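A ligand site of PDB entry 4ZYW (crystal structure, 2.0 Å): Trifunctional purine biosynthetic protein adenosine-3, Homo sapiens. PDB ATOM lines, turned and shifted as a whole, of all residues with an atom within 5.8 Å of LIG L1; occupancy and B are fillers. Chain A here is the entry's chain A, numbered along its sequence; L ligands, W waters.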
ATOM      1  N   GLY A  10      33.089  -6.123 -15.441  1.00  0.00           N
ATOM      2  CA  GLY A  10      33.733  -5.737 -14.196  1.00  0.00           C
ATOM      3  C   GLY A  10      35.003  -6.470 -13.795  1.00  0.00           C
ATOM      4  O   GLY A  10      35.957  -6.533 -14.567  1.00  0.00           O
ATOM      5  N   THR A  11      34.991  -7.037 -12.587  1.00  0.00           N
ATOM      6  CA  THR A  11      36.192  -7.587 -11.949  1.00  0.00           C
ATOM      7  C   THR A  11      36.914  -8.627 -12.818  1.00  0.00           C
ATOM      8  O   THR A  11      38.131  -8.554 -12.985  1.00  0.00           O
ATOM      9  CB  THR A  11      35.847  -8.251 -10.579  1.00  0.00           C
ATOM     10  OG1 THR A  11      35.122  -7.329  -9.754  1.00  0.00           O
ATOM     11  CG2 THR A  11      37.119  -8.680  -9.861  1.00  0.00           C
ATOM     12  N   GLY A  12      36.172  -9.599 -13.341  1.00  0.00           N
ATOM     13  CA  GLY A  12      36.750 -10.595 -14.217  1.00  0.00           C
ATOM     14  C   GLY A  12      37.390 -11.794 -13.545  1.00  0.00           C
ATOM     15  O   GLY A  12      38.316 -12.396 -14.108  1.00  0.00           O
ATOM     16  N   SER A  13      36.890 -12.195 -12.368  1.00  0.00           N
ATOM     17  CA  SER A  13      37.410 -13.415 -11.744  1.00  0.00           C
ATOM     18  C   SER A  13      37.011 -14.645 -12.596  1.00  0.00           C
ATOM     19  O   SER A  13      37.797 -15.585 -12.735  1.00  0.00           O
ATOM     20  CB  SER A  13      36.911 -13.573 -10.306  1.00  0.00           C
ATOM     21  OG  SER A  13      35.521 -13.838 -10.258  1.00  0.00           O
ATOM     22  N   ASN A  14      35.815 -14.630 -13.181  1.00  0.00           N
ATOM     23  CA  ASN A  14      35.432 -15.734 -14.065  1.00  0.00           C
ATOM     24  C   ASN A  14      36.282 -15.760 -15.322  1.00  0.00           C
ATOM     25  O   ASN A  14      36.710 -16.832 -15.774  1.00  0.00           O
ATOM     26  CB  ASN A  14      33.947 -15.660 -14.432  1.00  0.00           C
ATOM     27  CG  ASN A  14      33.066 -16.355 -13.407  1.00  0.00           C
ATOM     28  OD1 ASN A  14      33.002 -17.591 -13.351  1.00  0.00           O
ATOM     29  ND2 ASN A  14      32.375 -15.572 -12.588  1.00  0.00           N
ATOM     30  N   LEU A  15      36.559 -14.588 -15.889  1.00  0.00           N
ATOM     31  CA  LEU A  15      37.500 -14.487 -17.012  1.00  0.00           C
ATOM     32  C   LEU A  15      38.859 -15.104 -16.671  1.00  0.00           C
ATOM     33  O   LEU A  15      39.407 -15.890 -17.455  1.00  0.00           O
ATOM     34  CB  LEU A  15      37.709 -13.020 -17.424  1.00  0.00           C
ATOM     35  CG  LEU A  15      38.896 -12.788 -18.377  1.00  0.00           C
ATOM     36  CD1 LEU A  15      38.673 -13.496 -19.708  1.00  0.00           C
ATOM     37  CD2 LEU A  15      39.127 -11.280 -18.602  1.00  0.00           C
ATOM     38  N   ALA A  87      30.769 -13.411 -19.047  1.00  0.00           N
ATOM     39  CA  ALA A  87      31.436 -13.626 -17.765  1.00  0.00           C
ATOM     40  C   ALA A  87      31.378 -12.372 -16.913  1.00  0.00           C
ATOM     41  O   ALA A  87      32.299 -11.558 -16.902  1.00  0.00           O
ATOM     42  CB  ALA A  87      32.898 -14.031 -17.981  1.00  0.00           C
ATOM     43  N   GLY A  88      30.261 -12.210 -16.207  1.00  0.00           N
ATOM     44  CA  GLY A  88      30.006 -10.981 -15.473  1.00  0.00           C
ATOM     45  C   GLY A  88      29.552  -9.875 -16.401  1.00  0.00           C
ATOM     46  O   GLY A  88      29.597  -8.699 -16.042  1.00  0.00           O
ATOM     47  N   PHE A  89      29.116 -10.252 -17.601  1.00  0.00           N
ATOM     48  CA  PHE A  89      28.585  -9.294 -18.568  1.00  0.00           C
ATOM     49  C   PHE A  89      27.159  -8.936 -18.192  1.00  0.00           C
ATOM     50  O   PHE A  89      26.280  -9.794 -18.222  1.00  0.00           O
ATOM     51  CB  PHE A  89      28.647  -9.877 -19.985  1.00  0.00           C
ATOM     52  CG  PHE A  89      28.219  -8.912 -21.073  1.00  0.00           C
ATOM     53  CD1 PHE A  89      29.067  -7.899 -21.495  1.00  0.00           C
ATOM     54  CD2 PHE A  89      26.981  -9.046 -21.683  1.00  0.00           C
ATOM     55  CE1 PHE A  89      28.685  -7.025 -22.501  1.00  0.00           C
ATOM     56  CE2 PHE A  89      26.589  -8.176 -22.687  1.00  0.00           C
ATOM     57  CZ  PHE A  89      27.438  -7.162 -23.110  1.00  0.00           C
ATOM     58  N   MET A  90      26.916  -7.692 -17.821  1.00  0.00           N
ATOM     59  CA  MET A  90      25.602  -7.331 -17.303  1.00  0.00           C
ATOM     60  C   MET A  90      24.752  -6.555 -18.291  1.00  0.00           C
ATOM     61  O   MET A  90      24.198  -5.509 -17.931  1.00  0.00           O
ATOM     62  CB  MET A  90      25.750  -6.514 -16.006  1.00  0.00           C
ATOM     63  CG  MET A  90      26.544  -7.221 -14.910  1.00  0.00           C
ATOM     64  SD  MET A  90      25.855  -8.832 -14.403  1.00  0.00           S
ATOM     65  CE  MET A  90      24.442  -8.300 -13.427  1.00  0.00           C
ATOM     66  N   ASN A 107      26.456 -18.425 -20.644  1.00  0.00           N
ATOM     67  CA  ASN A 107      26.393 -17.451 -19.568  1.00  0.00           C
ATOM     68  C   ASN A 107      26.565 -18.139 -18.222  1.00  0.00           C
ATOM     69  O   ASN A 107      26.076 -19.251 -18.050  1.00  0.00           O
ATOM     70  CB  ASN A 107      25.051 -16.700 -19.591  1.00  0.00           C
ATOM     71  CG  ASN A 107      24.923 -15.664 -18.473  1.00  0.00           C
ATOM     72  OD1 ASN A 107      25.762 -14.770 -18.360  1.00  0.00           O
ATOM     73  ND2 ASN A 107      23.872 -15.780 -17.674  1.00  0.00           N
ATOM     74  N   ILE A 108      27.282 -17.505 -17.297  1.00  0.00           N
ATOM     75  CA  ILE A 108      27.302 -17.957 -15.889  1.00  0.00           C
ATOM     76  C   ILE A 108      26.333 -17.103 -15.061  1.00  0.00           C
ATOM     77  O   ILE A 108      26.273 -15.870 -15.212  1.00  0.00           O
ATOM     78  CB  ILE A 108      28.739 -17.910 -15.279  1.00  0.00           C
ATOM     79  CG1 ILE A 108      28.751 -18.447 -13.842  1.00  0.00           C
ATOM     80  CG2 ILE A 108      29.283 -16.482 -15.294  1.00  0.00           C
ATOM     81  CD1 ILE A 108      28.895 -19.953 -13.719  1.00  0.00           C
ATOM     82  N   HIS A 109      25.565 -17.758 -14.212  1.00  0.00           N
ATOM     83  CA  HIS A 109      24.564 -17.096 -13.382  1.00  0.00           C
ATOM     84  C   HIS A 109      24.666 -17.627 -11.959  1.00  0.00           C
ATOM     85  O   HIS A 109      24.698 -18.843 -11.760  1.00  0.00           O
ATOM     86  CB  HIS A 109      23.159 -17.307 -13.935  1.00  0.00           C
ATOM     87  CG  HIS A 109      22.086 -16.611 -13.139  1.00  0.00           C
ATOM     88  ND1 HIS A 109      21.787 -15.280 -13.308  1.00  0.00           N
ATOM     89  CD2 HIS A 109      21.276 -17.061 -12.160  1.00  0.00           C
ATOM     90  CE1 HIS A 109      20.815 -14.935 -12.479  1.00  0.00           C
ATOM     91  NE2 HIS A 109      20.497 -15.996 -11.769  1.00  0.00           N
ATOM     92  N   PRO A 110      24.716 -16.709 -10.952  1.00  0.00           N
ATOM     93  CA  PRO A 110      25.006 -17.111  -9.559  1.00  0.00           C
ATOM     94  C   PRO A 110      23.759 -17.529  -8.797  1.00  0.00           C
ATOM     95  O   PRO A 110      23.526 -17.079  -7.667  1.00  0.00           O
ATOM     96  CB  PRO A 110      25.626 -15.847  -8.950  1.00  0.00           C
ATOM     97  CG  PRO A 110      24.929 -14.733  -9.675  1.00  0.00           C
ATOM     98  CD  PRO A 110      24.710 -15.254 -11.112  1.00  0.00           C
ATOM     99  N   GLY A 118      17.801 -12.917 -12.856  1.00  0.00           N
ATOM    100  CA  GLY A 118      17.981 -11.481 -12.800  1.00  0.00           C
ATOM    101  C   GLY A 118      19.348 -11.049 -12.292  1.00  0.00           C
ATOM    102  O   GLY A 118      20.239 -11.884 -12.141  1.00  0.00           O
ATOM    103  N   SER A 119      19.511  -9.759 -12.014  1.00  0.00           N
ATOM    104  CA  SER A 119      20.832  -9.217 -11.718  1.00  0.00           C
ATOM    105  C   SER A 119      21.237  -9.237 -10.245  1.00  0.00           C
ATOM    106  O   SER A 119      22.398  -8.937  -9.918  1.00  0.00           O
ATOM    107  CB  SER A 119      20.925  -7.778 -12.233  1.00  0.00           C
ATOM    108  OG  SER A 119      20.042  -6.945 -11.496  1.00  0.00           O
ATOM    109  N   HIS A 122      21.845 -13.088  -5.493  1.00  0.00           N
ATOM    110  CA  HIS A 122      22.225 -13.307  -4.096  1.00  0.00           C
ATOM    111  C   HIS A 122      21.271 -12.603  -3.113  1.00  0.00           C
ATOM    112  O   HIS A 122      20.903 -13.164  -2.081  1.00  0.00           O
ATOM    113  CB  HIS A 122      23.661 -12.843  -3.843  1.00  0.00           C
ATOM    114  CG  HIS A 122      24.703 -13.618  -4.602  1.00  0.00           C
ATOM    115  ND1 HIS A 122      24.774 -14.985  -4.567  1.00  0.00           N
ATOM    116  CD2 HIS A 122      25.706 -13.202  -5.414  1.00  0.00           C
ATOM    117  CE1 HIS A 122      25.781 -15.393  -5.321  1.00  0.00           C
ATOM    118  NE2 HIS A 122      26.370 -14.329  -5.839  1.00  0.00           N
ATOM    119  N   ASP A 145      18.093 -15.885 -18.712  1.00  0.00           N
ATOM    120  CA  ASP A 145      18.327 -16.928 -17.708  1.00  0.00           C
ATOM    121  C   ASP A 145      17.392 -18.115 -17.875  1.00  0.00           C
ATOM    122  O   ASP A 145      17.118 -18.842 -16.913  1.00  0.00           O
ATOM    123  CB  ASP A 145      18.211 -16.344 -16.293  1.00  0.00           C
ATOM    124  CG  ASP A 145      19.251 -15.268 -15.995  1.00  0.00           C
ATOM    125  OD1 ASP A 145      20.349 -15.260 -16.620  1.00  0.00           O
ATOM    126  OD2 ASP A 145      18.989 -14.419 -15.116  1.00  0.00           O
ATOM    127  N   SER A 167      28.488 -14.409  -2.148  1.00  0.00           N
ATOM    128  CA  SER A 167      28.985 -14.342  -3.528  1.00  0.00           C
ATOM    129  C   SER A 167      30.432 -14.829  -3.622  1.00  0.00           C
ATOM    130  O   SER A 167      30.843 -15.401  -4.650  1.00  0.00           O
ATOM    131  CB  SER A 167      28.878 -12.925  -4.115  1.00  0.00           C
ATOM    132  OG  SER A 167      29.675 -12.010  -3.401  1.00  0.00           O
ATOM    133  N   LYS A 171      31.363 -17.821  -6.048  1.00  0.00           N
ATOM    134  CA  LYS A 171      32.379 -17.607  -7.087  1.00  0.00           C
ATOM    135  C   LYS A 171      33.393 -18.776  -7.149  1.00  0.00           C
ATOM    136  O   LYS A 171      33.878 -19.117  -8.226  1.00  0.00           O
ATOM    137  CB  LYS A 171      33.116 -16.282  -6.881  1.00  0.00           C
ATOM    138  CG  LYS A 171      32.335 -15.107  -7.492  1.00  0.00           C
ATOM    139  CD  LYS A 171      33.102 -13.780  -7.464  1.00  0.00           C
ATOM    140  CE  LYS A 171      32.209 -12.632  -7.977  1.00  0.00           C
ATOM    141  NZ  LYS A 171      32.995 -11.368  -8.240  1.00  0.00           N
ATOM    142  N   GLU A 174      31.654 -21.098  -9.345  1.00  0.00           N
ATOM    143  CA  GLU A 174      31.602 -20.549 -10.696  1.00  0.00           C
ATOM    144  C   GLU A 174      32.885 -20.825 -11.458  1.00  0.00           C
ATOM    145  O   GLU A 174      32.857 -21.167 -12.650  1.00  0.00           O
ATOM    146  CB  GLU A 174      31.354 -19.041 -10.681  1.00  0.00           C
ATOM    147  CG  GLU A 174      30.019 -18.622 -10.117  1.00  0.00           C
ATOM    148  CD  GLU A 174      29.814 -17.101 -10.192  1.00  0.00           C
ATOM    149  OE1 GLU A 174      30.195 -16.473 -11.207  1.00  0.00           O
ATOM    150  OE2 GLU A 174      29.273 -16.521  -9.219  1.00  0.00           O
ATOM    151  N   HIS A 175      34.010 -20.685 -10.758  1.00  0.00           N
ATOM    152  CA  HIS A 175      35.319 -20.799 -11.385  1.00  0.00           C
ATOM    153  C   HIS A 175      35.646 -22.243 -11.711  1.00  0.00           C
ATOM    154  O   HIS A 175      36.632 -22.515 -12.397  1.00  0.00           O
ATOM    155  CB  HIS A 175      36.411 -20.220 -10.490  1.00  0.00           C
ATOM    156  CG  HIS A 175      36.244 -18.767 -10.202  1.00  0.00           C
ATOM    157  ND1 HIS A 175      36.861 -18.143  -9.143  1.00  0.00           N
ATOM    158  CD2 HIS A 175      35.529 -17.809 -10.842  1.00  0.00           C
ATOM    159  CE1 HIS A 175      36.537 -16.865  -9.138  1.00  0.00           C
ATOM    160  NE2 HIS A 175      35.723 -16.638 -10.157  1.00  0.00           N
HETATM  161  C1  LIG L   1      29.584 -13.457 -11.060  1.00  0.00           C
HETATM  162  O1  LIG L   1      29.152 -13.853  -9.743  1.00  0.00           O
HETATM  163  C2  LIG L   1      28.519 -13.857 -12.068  1.00  0.00           C
HETATM  164  O2  LIG L   1      27.872 -15.105 -11.778  1.00  0.00           O
HETATM  165  C3  LIG L   1      27.539 -12.695 -12.001  1.00  0.00           C
HETATM  166  O3  LIG L   1      28.382 -11.560 -11.850  1.00  0.00           O
HETATM  167  C4  LIG L   1      29.613 -11.931 -11.193  1.00  0.00           C
HETATM  168  C5  LIG L   1      30.799 -11.430 -12.021  1.00  0.00           C
HETATM  169  O4  LIG L   1      32.031 -11.579 -11.314  1.00  0.00           O
HETATM  170  N1  LIG L   1      26.730 -12.622 -13.207  1.00  0.00           N
HETATM  171  C6  LIG L   1      25.437 -12.282 -13.172  1.00  0.00           C
HETATM  172  O5  LIG L   1      24.868 -11.906 -12.142  1.00  0.00           O
HETATM  173  C7  LIG L   1      24.713 -12.374 -14.497  1.00  0.00           C
HETATM  174  N2  LIG L   1      23.367 -11.816 -14.422  1.00  0.00           N
HETATM  175  P1  LIG L   1      33.465 -11.544 -12.092  1.00  0.00           P
HETATM  176  O6  LIG L   1      33.394 -12.743 -13.028  1.00  0.00           O
HETATM  177  O7  LIG L   1      34.505 -11.635 -11.000  1.00  0.00           O
HETATM  178  O8  LIG L   1      33.506 -10.211 -12.836  1.00  0.00           O
HETATM  179  N1  LG2 L   2      20.578 -11.818 -22.684  1.00  0.00           N
HETATM  180  C1  LG2 L   2      19.670 -12.666 -23.134  1.00  0.00           C
HETATM  181  N2  LG2 L   2      19.480 -13.868 -22.558  1.00  0.00           N
HETATM  182  C2  LG2 L   2      20.178 -14.258 -21.473  1.00  0.00           C
HETATM  183  N3  LG2 L   2      22.287 -11.417 -20.992  1.00  0.00           N
HETATM  184  C3  LG2 L   2      22.763 -12.104 -19.960  1.00  0.00           C
HETATM  185  C4  LG2 L   2      22.092 -13.361 -19.866  1.00  0.00           C
HETATM  186  C5  LG2 L   2      21.158 -13.361 -20.957  1.00  0.00           C
HETATM  187  C6  LG2 L   2      21.339 -12.111 -21.611  1.00  0.00           C
HETATM  188  O1  LG2 L   2      19.918 -15.535 -20.886  1.00  0.00           O
HETATM  189  N4  LG2 L   2      18.892 -12.344 -24.249  1.00  0.00           N
HETATM  190  S1  LG2 L   2      21.735  -7.943 -16.925  1.00  0.00           S
HETATM  191  C7  LG2 L   2      20.498  -7.284 -15.932  1.00  0.00           C
HETATM  192  C8  LG2 L   2      19.642  -8.380 -15.634  1.00  0.00           C
HETATM  193  C9  LG2 L   2      20.035  -9.649 -16.211  1.00  0.00           C
HETATM  194  C10 LG2 L   2      21.227  -9.554 -16.983  1.00  0.00           C
HETATM  195  C11 LG2 L   2      20.177  -5.870 -15.338  1.00  0.00           C
HETATM  196  O2  LG2 L   2      19.139  -5.795 -14.647  1.00  0.00           O
HETATM  197  N5  LG2 L   2      20.889  -4.609 -15.434  1.00  0.00           N
HETATM  198  C12 LG2 L   2      22.103  -4.278 -16.130  1.00  0.00           C
HETATM  199  C13 LG2 L   2      21.747  -3.213 -17.114  1.00  0.00           C
HETATM  200  C14 LG2 L   2      21.904  -3.648 -18.563  1.00  0.00           C
HETATM  201  C15 LG2 L   2      20.702  -4.409 -19.168  1.00  0.00           C
HETATM  202  O3  LG2 L   2      20.573  -4.498 -20.450  1.00  0.00           O
HETATM  203  O4  LG2 L   2      19.819  -4.981 -18.386  1.00  0.00           O
HETATM  204  C16 LG2 L   2      23.109  -3.672 -15.135  1.00  0.00           C
HETATM  205  O5  LG2 L   2      23.839  -4.435 -14.359  1.00  0.00           O
HETATM  206  O6  LG2 L   2      23.245  -2.399 -15.084  1.00  0.00           O
HETATM  207  C17 LG2 L   2      23.880 -11.601 -19.005  1.00  0.00           C
HETATM  208  C18 LG2 L   2      23.340 -10.556 -17.958  1.00  0.00           C
HETATM  209  C19 LG2 L   2      21.847 -10.741 -17.691  1.00  0.00           C
HETATM  210  O   HOH W   1      28.133 -12.474  -7.816  1.00  0.00           O
HETATM  211  O   HOH W   2      27.784 -13.619 -15.634  1.00  0.00           O
HETATM  212  O   HOH W   3      34.515 -12.413 -15.450  1.00  0.00           O
HETATM  213  O   HOH W   4      28.819 -15.277  -6.867  1.00  0.00           O
HETATM  214  O   HOH W   5      22.561 -12.067 -10.485  1.00  0.00           O
HETATM  215  O   HOH W   6      32.934  -9.220 -15.314  1.00  0.00           O
HETATM  216  O   HOH W   7      22.410 -14.067 -15.586  1.00  0.00           O
HETATM  217  O   HOH W   8      25.805 -10.364 -10.225  1.00  0.00           O
HETATM  218  O   HOH W   9      32.138  -8.179 -11.787  1.00  0.00           O
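An oxygen (O7) of LIG L1 lies within hydrogen-bond range of the backbone NH (N) of Ser 13 (2.8 Å).
The side-chain hydroxyl (OG) of Ser 13 is in hydrogen-bond range of an oxygen (O7) of LIG L1 (2.5 Å).
The side-chain carboxylate (OE2) of Glu 174 is in hydrogen-bond range of an oxygen (O1) of LIG L1 (2.7 Å).
The backbone NH of Gly 12 is in hydrogen-bond range of an oxygen (O8) of LIG L1 (2.8 Å).
N of Asn 14 sits at hydrogen-bond distance from O6 of LIG L1, 3.1 Å away.
ND2 of Asn 14 is in hydrogen-bond range of O6 of LIG L1.
NZ of Lys 171 lies within salt-bridge range of O7 of LIG L1.
An oxygen (O2) of LG2 L2 lies within hydrogen-bond range of the side-chain hydroxyl (OG) of Ser 119, at 3.5 Å.
N of Asp 145 lies within hydrogen-bond range of O1 of LG2 L2 (2.9 Å).
Residues that only touch LIG L1: Pro 110 (3.2 Å), Thr 11 (3.5 Å), Gly 88 (3.6 Å), Met 90 (3.7 Å), Ile 108 (3.8 Å), Gly 118 (3.9 Å) and His 109 (3.97 Å).
Hydrophobic or aromatic side chains within 4 Å of LIG L1: Met 90 and Pro 110.
12 residues have an atom within 4 Å of LIG L1: Thr 11, Gly 12, Ser 13, Asn 14, Gly 88, Met 90, Ile 108, His 109, Pro 110, Gly 118, Lys 171 and Glu 174.
Along chain A the residues within 4 Å of LIG L1 span positions 11 to 174.
NE2 of His 175 is in hydrogen-bond range of OG of Ser 13 (2.8 Å).
The side-chain carboxylate (OE1) of Glu 174 is in hydrogen-bond range of the side-chain amide nitrogen (ND2) of Asn 14 (2.7 Å).
The backbone carbonyl oxygen of Lys 171 lies close to a ring nitrogen (ND1) of His 175 (3.3 Å).
The side-chain carboxylate of Asp 145 is in hydrogen-bond range of the backbone NH of Gly 118 (3.0 Å).
OD2 of Asp 145 lies close to ND1 of His 109 (3.4 Å).
Water W1 bridges O1 of LIG L1 and NE2 of His 122.
Water W9 lies within hydrogen-bond range of an oxygen (O8) of LIG L1 (2.7 Å) and the backbone NH of Thr 11 (3.2 Å).
Water W3 lies within hydrogen-bond range of an oxygen (O6) of LIG L1 (2.7 Å), the backbone carbonyl oxygen of Ala 87 (2.8 Å), the backbone NH of Leu 15 (3.0 Å) and the backbone NH of Asn 14 (3.4 Å).
Water W7 lies within hydrogen-bond range of the side-chain carboxylate (OD1) of Asp 145 (2.6 Å), a ring nitrogen (ND1) of His 109 (2.7 Å), a nitrogen (N2) of LIG L1 (2.7 Å) and the side-chain amide nitrogen (ND2) of Asn 107 (3.1 Å).
Water W6 lies within hydrogen-bond range of an oxygen (O8) of LIG L1 (2.7 Å), the backbone carbonyl oxygen of Ala 87 (2.9 Å), the backbone NH of Gly 10 (3.1 Å) and the backbone carbonyl oxygen of Gly 88 (3.5 Å).
Water W4 lies within hydrogen-bond range of the side-chain carboxylate (OE2) of Glu 174, a ring nitrogen (NE2) of His 122, the backbone carbonyl oxygen (O) of Ser 167 and an oxygen (O1) of LIG L1.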
